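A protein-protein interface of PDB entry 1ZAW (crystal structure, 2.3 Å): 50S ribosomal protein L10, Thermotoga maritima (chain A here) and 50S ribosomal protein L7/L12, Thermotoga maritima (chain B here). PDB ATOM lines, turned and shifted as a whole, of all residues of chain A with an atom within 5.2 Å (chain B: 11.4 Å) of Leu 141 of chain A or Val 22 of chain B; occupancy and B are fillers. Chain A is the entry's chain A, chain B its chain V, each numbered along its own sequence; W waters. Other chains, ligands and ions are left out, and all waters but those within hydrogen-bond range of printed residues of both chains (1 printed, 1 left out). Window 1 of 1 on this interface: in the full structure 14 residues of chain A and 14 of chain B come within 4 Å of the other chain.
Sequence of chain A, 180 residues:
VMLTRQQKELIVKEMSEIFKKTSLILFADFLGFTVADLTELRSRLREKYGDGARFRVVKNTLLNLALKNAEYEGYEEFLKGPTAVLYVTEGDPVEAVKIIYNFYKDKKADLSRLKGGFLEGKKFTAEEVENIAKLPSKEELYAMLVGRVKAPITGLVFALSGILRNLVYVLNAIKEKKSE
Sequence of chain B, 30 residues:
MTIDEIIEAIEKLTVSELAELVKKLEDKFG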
ATOM      1  N   PRO A 136      21.654   2.341 -17.143  1.00  0.00           N
ATOM      2  CA  PRO A 136      22.863   2.564 -17.947  1.00  0.00           C
ATOM      3  C   PRO A 136      22.679   1.983 -19.343  1.00  0.00           C
ATOM      4  O   PRO A 136      21.663   1.360 -19.619  1.00  0.00           O
ATOM      5  CB  PRO A 136      23.954   1.857 -17.141  1.00  0.00           C
ATOM      6  CG  PRO A 136      23.195   0.782 -16.388  1.00  0.00           C
ATOM      7  CD  PRO A 136      21.920   1.463 -15.989  1.00  0.00           C
ATOM      8  N   SER A 137      23.646   2.189 -20.227  1.00  0.00           N
ATOM      9  CA  SER A 137      23.513   1.669 -21.579  1.00  0.00           C
ATOM     10  C   SER A 137      23.742   0.160 -21.633  1.00  0.00           C
ATOM     11  O   SER A 137      24.294  -0.442 -20.706  1.00  0.00           O
ATOM     12  CB  SER A 137      24.492   2.374 -22.527  1.00  0.00           C
ATOM     13  OG  SER A 137      25.837   2.072 -22.204  1.00  0.00           O
ATOM     14  N   LYS A 138      23.316  -0.449 -22.733  1.00  0.00           N
ATOM     15  CA  LYS A 138      23.486  -1.878 -22.904  1.00  0.00           C
ATOM     16  C   LYS A 138      24.964  -2.216 -22.746  1.00  0.00           C
ATOM     17  O   LYS A 138      25.323  -3.192 -22.086  1.00  0.00           O
ATOM     18  CB  LYS A 138      22.996  -2.296 -24.286  1.00  0.00           C
ATOM     19  CG  LYS A 138      22.846  -3.786 -24.458  1.00  0.00           C
ATOM     20  CD  LYS A 138      22.070  -4.102 -25.720  1.00  0.00           C
ATOM     21  CE  LYS A 138      21.403  -5.458 -25.627  1.00  0.00           C
ATOM     22  NZ  LYS A 138      20.516  -5.703 -26.797  1.00  0.00           N
ATOM     23  N   GLU A 139      25.818  -1.393 -23.344  1.00  0.00           N
ATOM     24  CA  GLU A 139      27.261  -1.600 -23.277  1.00  0.00           C
ATOM     25  C   GLU A 139      27.757  -1.578 -21.827  1.00  0.00           C
ATOM     26  O   GLU A 139      28.533  -2.433 -21.416  1.00  0.00           O
ATOM     27  CB  GLU A 139      27.978  -0.519 -24.091  1.00  0.00           C
ATOM     28  CG  GLU A 139      27.268  -0.139 -25.397  1.00  0.00           C
ATOM     29  CD  GLU A 139      26.954  -1.343 -26.280  1.00  0.00           C
ATOM     30  OE1 GLU A 139      27.876  -2.150 -26.543  1.00  0.00           O
ATOM     31  OE2 GLU A 139      25.785  -1.478 -26.715  1.00  0.00           O
ATOM     32  N   GLU A 140      27.301  -0.597 -21.058  1.00  0.00           N
ATOM     33  CA  GLU A 140      27.694  -0.479 -19.660  1.00  0.00           C
ATOM     34  C   GLU A 140      27.213  -1.677 -18.843  1.00  0.00           C
ATOM     35  O   GLU A 140      27.960  -2.209 -18.024  1.00  0.00           O
ATOM     36  CB  GLU A 140      27.136   0.813 -19.056  1.00  0.00           C
ATOM     37  CG  GLU A 140      27.648   2.076 -19.728  1.00  0.00           C
ATOM     38  CD  GLU A 140      27.136   3.348 -19.062  1.00  0.00           C
ATOM     39  OE1 GLU A 140      25.905   3.568 -19.036  1.00  0.00           O
ATOM     40  OE2 GLU A 140      27.969   4.131 -18.558  1.00  0.00           O
ATOM     41  N   LEU A 141      25.964  -2.085 -19.059  1.00  0.00           N
ATOM     42  CA  LEU A 141      25.409  -3.228 -18.352  1.00  0.00           C
ATOM     43  C   LEU A 141      26.176  -4.496 -18.677  1.00  0.00           C
ATOM     44  O   LEU A 141      26.313  -5.369 -17.827  1.00  0.00           O
ATOM     45  CB  LEU A 141      23.939  -3.429 -18.708  1.00  0.00           C
ATOM     46  CG  LEU A 141      22.929  -2.464 -18.083  1.00  0.00           C
ATOM     47  CD1 LEU A 141      21.611  -2.580 -18.836  1.00  0.00           C
ATOM     48  CD2 LEU A 141      22.752  -2.761 -16.599  1.00  0.00           C
ATOM     49  N   TYR A 142      26.676  -4.606 -19.905  1.00  0.00           N
ATOM     50  CA  TYR A 142      27.434  -5.790 -20.284  1.00  0.00           C
ATOM     51  C   TYR A 142      28.717  -5.824 -19.479  1.00  0.00           C
ATOM     52  O   TYR A 142      29.133  -6.882 -19.009  1.00  0.00           O
ATOM     53  CB  TYR A 142      27.781  -5.768 -21.765  1.00  0.00           C
ATOM     54  CG  TYR A 142      26.740  -6.372 -22.673  1.00  0.00           C
ATOM     55  CD1 TYR A 142      26.490  -5.812 -23.923  1.00  0.00           C
ATOM     56  CD2 TYR A 142      26.033  -7.519 -22.311  1.00  0.00           C
ATOM     57  CE1 TYR A 142      25.567  -6.374 -24.794  1.00  0.00           C
ATOM     58  CE2 TYR A 142      25.102  -8.092 -23.179  1.00  0.00           C
ATOM     59  CZ  TYR A 142      24.879  -7.510 -24.422  1.00  0.00           C
ATOM     60  OH  TYR A 142      23.979  -8.047 -25.318  1.00  0.00           O
ATOM     61  N   ALA A 143      29.345  -4.658 -19.328  1.00  0.00           N
ATOM     62  CA  ALA A 143      30.584  -4.556 -18.564  1.00  0.00           C
ATOM     63  C   ALA A 143      30.319  -4.904 -17.109  1.00  0.00           C
ATOM     64  O   ALA A 143      31.099  -5.605 -16.476  1.00  0.00           O
ATOM     65  CB  ALA A 143      31.165  -3.147 -18.680  1.00  0.00           C
ATOM     66  N   MET A 144      29.211  -4.408 -16.578  1.00  0.00           N
ATOM     67  CA  MET A 144      28.836  -4.693 -15.204  1.00  0.00           C
ATOM     68  C   MET A 144      28.599  -6.192 -15.021  1.00  0.00           C
ATOM     69  O   MET A 144      28.971  -6.765 -14.001  1.00  0.00           O
ATOM     70  CB  MET A 144      27.564  -3.923 -14.845  1.00  0.00           C
ATOM     71  CG  MET A 144      27.818  -2.489 -14.488  1.00  0.00           C
ATOM     72  SD  MET A 144      26.141  -1.510 -14.318  1.00  0.00           S
ATOM     73  CE  MET A 144      25.508  -2.297 -12.696  1.00  0.00           C
ATOM     74  N   LEU A 145      27.971  -6.811 -16.016  1.00  0.00           N
ATOM     75  CA  LEU A 145      27.654  -8.226 -15.965  1.00  0.00           C
ATOM     76  C   LEU A 145      28.874  -9.088 -15.633  1.00  0.00           C
ATOM     77  O   LEU A 145      28.801  -9.969 -14.778  1.00  0.00           O
ATOM     78  CB  LEU A 145      27.033  -8.676 -17.297  1.00  0.00           C
ATOM     79  CG  LEU A 145      26.500 -10.115 -17.340  1.00  0.00           C
ATOM     80  CD1 LEU A 145      25.368 -10.280 -16.332  1.00  0.00           C
ATOM     81  CD2 LEU A 145      26.002 -10.445 -18.755  1.00  0.00           C
ATOM     82  N   ARG A 148      29.684  -9.160 -11.944  1.00  0.00           N
ATOM     83  CA  ARG A 148      28.666  -9.851 -11.154  1.00  0.00           C
ATOM     84  C   ARG A 148      28.707 -11.360 -11.326  1.00  0.00           C
ATOM     85  O   ARG A 148      28.380 -12.104 -10.401  1.00  0.00           O
ATOM     86  CB  ARG A 148      27.273  -9.345 -11.504  1.00  0.00           C
ATOM     87  CG  ARG A 148      26.882  -8.086 -10.768  1.00  0.00           C
ATOM     88  CD  ARG A 148      27.918  -7.001 -10.942  1.00  0.00           C
ATOM     89  NE  ARG A 148      27.452  -5.728 -10.412  1.00  0.00           N
ATOM     90  CZ  ARG A 148      28.045  -4.567 -10.657  1.00  0.00           C
ATOM     91  NH1 ARG A 148      27.555  -3.446 -10.138  1.00  0.00           N
ATOM     92  NH2 ARG A 148      29.131  -4.531 -11.423  1.00  0.00           N
ATOM     93  N   ALA B   9      22.106 -17.017 -24.618  1.00  0.00           N
ATOM     94  CA  ALA B   9      20.852 -16.585 -24.025  1.00  0.00           C
ATOM     95  C   ALA B   9      21.024 -15.187 -23.436  1.00  0.00           C
ATOM     96  O   ALA B   9      20.079 -14.408 -23.368  1.00  0.00           O
ATOM     97  CB  ALA B   9      20.424 -17.560 -22.944  1.00  0.00           C
ATOM     98  N   ILE B  10      22.242 -14.876 -23.022  1.00  0.00           N
ATOM     99  CA  ILE B  10      22.534 -13.586 -22.426  1.00  0.00           C
ATOM    100  C   ILE B  10      22.508 -12.465 -23.451  1.00  0.00           C
ATOM    101  O   ILE B  10      21.936 -11.403 -23.199  1.00  0.00           O
ATOM    102  CB  ILE B  10      23.918 -13.614 -21.711  1.00  0.00           C
ATOM    103  CG1 ILE B  10      23.757 -14.231 -20.318  1.00  0.00           C
ATOM    104  CG2 ILE B  10      24.538 -12.216 -21.668  1.00  0.00           C
ATOM    105  CD1 ILE B  10      25.061 -14.357 -19.550  1.00  0.00           C
ATOM    106  N   GLU B  11      23.112 -12.710 -24.611  1.00  0.00           N
ATOM    107  CA  GLU B  11      23.173 -11.704 -25.658  1.00  0.00           C
ATOM    108  C   GLU B  11      21.852 -11.431 -26.369  1.00  0.00           C
ATOM    109  O   GLU B  11      21.768 -10.508 -27.175  1.00  0.00           O
ATOM    110  CB  GLU B  11      24.250 -12.065 -26.680  1.00  0.00           C
ATOM    111  CG  GLU B  11      23.998 -13.344 -27.444  1.00  0.00           C
ATOM    112  CD  GLU B  11      25.082 -13.608 -28.480  1.00  0.00           C
ATOM    113  OE1 GLU B  11      26.278 -13.579 -28.102  1.00  0.00           O
ATOM    114  OE2 GLU B  11      24.741 -13.843 -29.663  1.00  0.00           O
ATOM    115  N   LEU B  13      19.144 -10.799 -24.609  1.00  0.00           N
ATOM    116  CA  LEU B  13      18.395 -10.037 -23.621  1.00  0.00           C
ATOM    117  C   LEU B  13      18.318  -8.554 -23.968  1.00  0.00           C
ATOM    118  O   LEU B  13      19.272  -7.961 -24.470  1.00  0.00           O
ATOM    119  CB  LEU B  13      19.038 -10.185 -22.233  1.00  0.00           C
ATOM    120  CG  LEU B  13      19.116 -11.574 -21.591  1.00  0.00           C
ATOM    121  CD1 LEU B  13      19.678 -11.446 -20.178  1.00  0.00           C
ATOM    122  CD2 LEU B  13      17.734 -12.214 -21.557  1.00  0.00           C
ATOM    123  N   THR B  14      17.172  -7.954 -23.695  1.00  0.00           N
ATOM    124  CA  THR B  14      16.999  -6.532 -23.946  1.00  0.00           C
ATOM    125  C   THR B  14      17.764  -5.759 -22.864  1.00  0.00           C
ATOM    126  O   THR B  14      18.308  -6.359 -21.926  1.00  0.00           O
ATOM    127  CB  THR B  14      15.532  -6.145 -23.870  1.00  0.00           C
ATOM    128  OG1 THR B  14      15.026  -6.477 -22.569  1.00  0.00           O
ATOM    129  CG2 THR B  14      14.717  -6.900 -24.951  1.00  0.00           C
ATOM    130  N   VAL B  15      17.810  -4.439 -23.002  1.00  0.00           N
ATOM    131  CA  VAL B  15      18.487  -3.585 -22.030  1.00  0.00           C
ATOM    132  C   VAL B  15      17.831  -3.766 -20.660  1.00  0.00           C
ATOM    133  O   VAL B  15      18.499  -3.933 -19.637  1.00  0.00           O
ATOM    134  CB  VAL B  15      18.386  -2.097 -22.435  1.00  0.00           C
ATOM    135  CG1 VAL B  15      18.947  -1.213 -21.329  1.00  0.00           C
ATOM    136  CG2 VAL B  15      19.138  -1.866 -23.737  1.00  0.00           C
ATOM    137  N   SER B  16      16.510  -3.737 -20.659  1.00  0.00           N
ATOM    138  CA  SER B  16      15.737  -3.891 -19.446  1.00  0.00           C
ATOM    139  C   SER B  16      16.018  -5.247 -18.791  1.00  0.00           C
ATOM    140  O   SER B  16      16.221  -5.331 -17.581  1.00  0.00           O
ATOM    141  CB  SER B  16      14.251  -3.746 -19.785  1.00  0.00           C
ATOM    142  OG  SER B  16      13.458  -3.762 -18.612  1.00  0.00           O
ATOM    143  N   GLU B  17      16.036  -6.304 -19.598  1.00  0.00           N
ATOM    144  CA  GLU B  17      16.293  -7.659 -19.106  1.00  0.00           C
ATOM    145  C   GLU B  17      17.691  -7.837 -18.495  1.00  0.00           C
ATOM    146  O   GLU B  17      17.868  -8.588 -17.525  1.00  0.00           O
ATOM    147  CB  GLU B  17      16.081  -8.669 -20.239  1.00  0.00           C
ATOM    148  CG  GLU B  17      14.624  -9.039 -20.447  1.00  0.00           C
ATOM    149  CD  GLU B  17      14.363  -9.779 -21.761  1.00  0.00           C
ATOM    150  OE1 GLU B  17      13.256 -10.340 -21.896  1.00  0.00           O
ATOM    151  OE2 GLU B  17      15.241  -9.792 -22.659  1.00  0.00           O
ATOM    152  N   LEU B  18      18.675  -7.156 -19.076  1.00  0.00           N
ATOM    153  CA  LEU B  18      20.044  -7.208 -18.590  1.00  0.00           C
ATOM    154  C   LEU B  18      20.124  -6.588 -17.206  1.00  0.00           C
ATOM    155  O   LEU B  18      20.804  -7.110 -16.325  1.00  0.00           O
ATOM    156  CB  LEU B  18      20.977  -6.427 -19.507  1.00  0.00           C
ATOM    157  CG  LEU B  18      21.684  -7.108 -20.666  1.00  0.00           C
ATOM    158  CD1 LEU B  18      22.643  -6.086 -21.301  1.00  0.00           C
ATOM    159  CD2 LEU B  18      22.455  -8.322 -20.173  1.00  0.00           C
ATOM    160  N   ALA B  19      19.435  -5.462 -17.035  1.00  0.00           N
ATOM    161  CA  ALA B  19      19.411  -4.751 -15.764  1.00  0.00           C
ATOM    162  C   ALA B  19      18.782  -5.635 -14.689  1.00  0.00           C
ATOM    163  O   ALA B  19      19.240  -5.647 -13.550  1.00  0.00           O
ATOM    164  CB  ALA B  19      18.629  -3.444 -15.906  1.00  0.00           C
ATOM    165  N   GLU B  20      17.732  -6.373 -15.048  1.00  0.00           N
ATOM    166  CA  GLU B  20      17.086  -7.260 -14.087  1.00  0.00           C
ATOM    167  C   GLU B  20      18.061  -8.379 -13.714  1.00  0.00           C
ATOM    168  O   GLU B  20      18.196  -8.730 -12.549  1.00  0.00           O
ATOM    169  CB  GLU B  20      15.796  -7.863 -14.661  1.00  0.00           C
ATOM    170  CG  GLU B  20      14.991  -8.639 -13.614  1.00  0.00           C
ATOM    171  CD  GLU B  20      13.777  -9.374 -14.185  1.00  0.00           C
ATOM    172  OE1 GLU B  20      12.942  -8.729 -14.863  1.00  0.00           O
ATOM    173  OE2 GLU B  20      13.653 -10.600 -13.944  1.00  0.00           O
ATOM    174  N   LEU B  21      18.743  -8.923 -14.719  1.00  0.00           N
ATOM    175  CA  LEU B  21      19.724  -9.984 -14.518  1.00  0.00           C
ATOM    176  C   LEU B  21      20.895  -9.503 -13.644  1.00  0.00           C
ATOM    177  O   LEU B  21      21.297 -10.185 -12.708  1.00  0.00           O
ATOM    178  CB  LEU B  21      20.266 -10.467 -15.869  1.00  0.00           C
ATOM    179  CG  LEU B  21      21.441 -11.442 -15.788  1.00  0.00           C
ATOM    180  CD1 LEU B  21      20.993 -12.755 -15.142  1.00  0.00           C
ATOM    181  CD2 LEU B  21      21.997 -11.680 -17.168  1.00  0.00           C
ATOM    182  N   VAL B  22      21.445  -8.333 -13.960  1.00  0.00           N
ATOM    183  CA  VAL B  22      22.556  -7.780 -13.191  1.00  0.00           C
ATOM    184  C   VAL B  22      22.206  -7.597 -11.716  1.00  0.00           C
ATOM    185  O   VAL B  22      23.015  -7.907 -10.845  1.00  0.00           O
ATOM    186  CB  VAL B  22      23.036  -6.415 -13.772  1.00  0.00           C
ATOM    187  CG1 VAL B  22      23.902  -5.674 -12.765  1.00  0.00           C
ATOM    188  CG2 VAL B  22      23.841  -6.658 -15.039  1.00  0.00           C
ATOM    189  N   LYS B  23      21.000  -7.112 -11.439  1.00  0.00           N
ATOM    190  CA  LYS B  23      20.579  -6.894 -10.060  1.00  0.00           C
ATOM    191  C   LYS B  23      20.370  -8.193  -9.289  1.00  0.00           C
ATOM    192  O   LYS B  23      20.792  -8.294  -8.144  1.00  0.00           O
ATOM    193  CB  LYS B  23      19.307  -6.047 -10.010  1.00  0.00           C
ATOM    194  CG  LYS B  23      19.486  -4.652 -10.578  1.00  0.00           C
ATOM    195  CD  LYS B  23      18.233  -3.797 -10.394  1.00  0.00           C
ATOM    196  CE  LYS B  23      18.430  -2.400 -10.981  1.00  0.00           C
ATOM    197  NZ  LYS B  23      19.663  -1.723 -10.446  1.00  0.00           N
ATOM    198  N   LYS B  24      19.710  -9.176  -9.897  1.00  0.00           N
ATOM    199  CA  LYS B  24      19.502 -10.445  -9.212  1.00  0.00           C
ATOM    200  C   LYS B  24      20.842 -11.119  -8.908  1.00  0.00           C
ATOM    201  O   LYS B  24      21.011 -11.733  -7.867  1.00  0.00           O
ATOM    202  CB  LYS B  24      18.630 -11.381 -10.053  1.00  0.00           C
ATOM    203  CG  LYS B  24      17.196 -10.930 -10.164  1.00  0.00           C
ATOM    204  CD  LYS B  24      16.310 -12.020 -10.737  1.00  0.00           C
ATOM    205  CE  LYS B  24      14.877 -11.534 -10.886  1.00  0.00           C
ATOM    206  NZ  LYS B  24      14.021 -12.495 -11.643  1.00  0.00           N
ATOM    207  N   LEU B  25      21.792 -10.991  -9.826  1.00  0.00           N
ATOM    208  CA  LEU B  25      23.120 -11.567  -9.663  1.00  0.00           C
ATOM    209  C   LEU B  25      23.878 -10.848  -8.544  1.00  0.00           C
ATOM    210  O   LEU B  25      24.716 -11.436  -7.844  1.00  0.00           O
ATOM    211  CB  LEU B  25      23.881 -11.445 -10.976  1.00  0.00           C
ATOM    212  CG  LEU B  25      24.395 -12.688 -11.715  1.00  0.00           C
ATOM    213  CD1 LEU B  25      23.567 -13.930 -11.429  1.00  0.00           C
ATOM    214  CD2 LEU B  25      24.399 -12.357 -13.192  1.00  0.00           C
ATOM    215  N   GLU B  26      23.573  -9.566  -8.391  1.00  0.00           N
ATOM    216  CA  GLU B  26      24.183  -8.727  -7.370  1.00  0.00           C
ATOM    217  C   GLU B  26      23.708  -9.221  -5.995  1.00  0.00           C
ATOM    218  O   GLU B  26      24.495  -9.375  -5.070  1.00  0.00           O
ATOM    219  CB  GLU B  26      23.745  -7.282  -7.602  1.00  0.00           C
ATOM    220  CG  GLU B  26      24.536  -6.207  -6.896  1.00  0.00           C
ATOM    221  CD  GLU B  26      23.942  -4.812  -7.137  1.00  0.00           C
ATOM    222  OE1 GLU B  26      23.553  -4.507  -8.293  1.00  0.00           O
ATOM    223  OE2 GLU B  26      23.872  -4.015  -6.170  1.00  0.00           O
ATOM    224  N   ASP B  27      22.413  -9.492  -5.883  1.00  0.00           N
ATOM    225  CA  ASP B  27      21.837  -9.955  -4.628  1.00  0.00           C
ATOM    226  C   ASP B  27      22.229 -11.382  -4.240  1.00  0.00           C
ATOM    227  O   ASP B  27      22.365 -11.686  -3.055  1.00  0.00           O
ATOM    228  CB  ASP B  27      20.313  -9.873  -4.685  1.00  0.00           C
ATOM    229  CG  ASP B  27      19.794  -8.449  -4.706  1.00  0.00           C
ATOM    230  OD1 ASP B  27      20.575  -7.505  -4.449  1.00  0.00           O
ATOM    231  OD2 ASP B  27      18.586  -8.283  -4.973  1.00  0.00           O
ATOM    232  N   LYS B  28      22.386 -12.258  -5.230  1.00  0.00           N
ATOM    233  CA  LYS B  28      22.748 -13.648  -4.966  1.00  0.00           C
ATOM    234  C   LYS B  28      24.210 -13.824  -4.623  1.00  0.00           C
ATOM    235  O   LYS B  28      24.550 -14.503  -3.653  1.00  0.00           O
ATOM    236  CB  LYS B  28      22.445 -14.538  -6.173  1.00  0.00           C
ATOM    237  CG  LYS B  28      20.983 -14.628  -6.540  1.00  0.00           C
ATOM    238  CD  LYS B  28      20.753 -15.695  -7.596  1.00  0.00           C
ATOM    239  CE  LYS B  28      20.814 -17.099  -6.994  1.00  0.00           C
ATOM    240  NZ  LYS B  28      19.579 -17.449  -6.219  1.00  0.00           N
ATOM    241  N   PHE B  29      25.075 -13.195  -5.417  1.00  0.00           N
ATOM    242  CA  PHE B  29      26.509 -13.341  -5.241  1.00  0.00           C
ATOM    243  C   PHE B  29      27.302 -12.210  -4.623  1.00  0.00           C
ATOM    244  O   PHE B  29      26.857 -11.070  -4.518  1.00  0.00           O
ATOM    245  CB  PHE B  29      27.146 -13.746  -6.581  1.00  0.00           C
ATOM    246  CG  PHE B  29      26.554 -14.998  -7.164  1.00  0.00           C
ATOM    247  CD1 PHE B  29      26.137 -15.034  -8.481  1.00  0.00           C
ATOM    248  CD2 PHE B  29      26.373 -16.134  -6.370  1.00  0.00           C
ATOM    249  CE1 PHE B  29      25.536 -16.184  -9.008  1.00  0.00           C
ATOM    250  CE2 PHE B  29      25.777 -17.284  -6.884  1.00  0.00           C
ATOM    251  CZ  PHE B  29      25.356 -17.311  -8.203  1.00  0.00           C
ATOM    252  N   GLY B  30      28.503 -12.596  -4.215  1.00  0.00           N
ATOM    253  CA  GLY B  30      29.467 -11.726  -3.581  1.00  0.00           C
ATOM    254  C   GLY B  30      30.603 -12.612  -3.082  1.00  0.00           C
ATOM    255  O   GLY B  30      30.547 -13.846  -3.325  1.00  0.00           O
ATOM    256  OXT GLY B  30      31.548 -12.090  -2.448  1.00  0.00           O
HETATM  257  O   HOH W   1      27.294 -10.688  -8.242  1.00  0.00           O
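Hydrophobic or aromatic side chains of chain B within 4 Å of the printed part of chain A: Ile 10, Val 15, Leu 18, Leu 21, Val 22 and Leu 25. Of the 11 printed residues of chain A, 6 touch a printed residue of chain B. Hydrophobic or aromatic side chains of chain A within 4 Å of the printed part of chain B: Leu 141, Tyr 142, Met 144 and Leu 145. Among the printed residues, 14 pairs touch across the chains. Among the printed residues, no Asp or Glu carboxylate lies within 4 Å of a Lys or Arg side-chain nitrogen of the other chain.
No residue of chain B comes within 4 Å of Pro 136 of chain A. No residue of chain B comes within 4 Å of Ser 137 of chain A. Of the printed residues of chain B, Lys 138 of chain A touches Leu 13 (3.5 Å), Val 15 (3.9 Å) and Leu 18 (3.9 Å). Printed residues of chain B within 4 Å of Leu 141 of chain A: Val 15, Leu 18, Ala 19 and Val 22. No residue of chain B comes within 4 Å of Ala 143 of chain A. Of chain B, only Val 22 (3.7 Å) comes within 4 Å of Met 144 of chain A. Of chain B, only Val 22 (3.9 Å) comes within 4 Å of Arg 148 of chain A. Ala 9 of chain B touches none of the printed residues of chain A. Printed residues of chain A within 4 Å of Ile 10 of chain B: Leu 145 (3.7 Å). Printed residues of chain A within 4 Å of Leu 13 of chain B: Lys 138 (3.5 Å). Thr 14 of chain B touches none of the printed residues of chain A. Of the printed residues of chain A, Leu 18 of chain B touches Lys 138 (3.9 Å), Leu 141 (3.9 Å) and Tyr 142 (3.7 Å). Printed residues of chain A within 4 Å of Leu 21 of chain B: Leu 145. Of chain A, only Leu 141 (3.9 Å), Met 144 (3.7 Å) and Arg 148 (3.9 Å) come within 4 Å of Val 22 of chain B. The nearest residue of chain B that does not touch Leu 141 of chain A is Ser 16 of chain B (5.5 Å). The nearest printed residue of chain A that does not touch Glu 11 of chain B is Lys 138 of chain A (5.0 Å).
The backbone carbonyl oxygen (O) of Leu 13 of chain B lies within hydrogen-bond range of the side-chain amino group (NZ) of Lys 138 of chain A (3.5 Å).
Water W1 bridges the backbone carbonyl oxygen of Leu 25 of chain B (2.7 Å) and the backbone carbonyl oxygen of Arg 148 of chain A (2.8 Å).
The backbone carbonyl oxygen of Met 144 of chain A sits close to the guanidinium group of Arg 148 of chain A (3.4 Å).
Among the printed residues, pairs that only touch across the chains: Lys 138 of chain A with Val 15 of chain B (3.9 Å), Lys 138 of chain A with Leu 18 of chain B (3.9 Å), Leu 141 of chain A with Val 15 of chain B (3.5 Å), Leu 141 of chain A with Leu 18 of chain B (3.9 Å), Leu 141 of chain A with Ala 19 of chain B (3.98 Å), Leu 141 of chain A with Val 22 of chain B (3.9 Å), Tyr 142 of chain A with Glu 11 of chain B (3.8 Å), Tyr 142 of chain A with Leu 18 of chain B (3.7 Å), Met 144 of chain A with Val 22 of chain B (3.7 Å), Leu 145 of chain A with Ile 10 of chain B (3.7 Å), Leu 145 of chain A with Leu 21 of chain B (3.7 Å), Leu 145 of chain A with Leu 25 of chain B (3.9 Å) and Arg 148 of chain A with Val 22 of chain B (3.9 Å).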
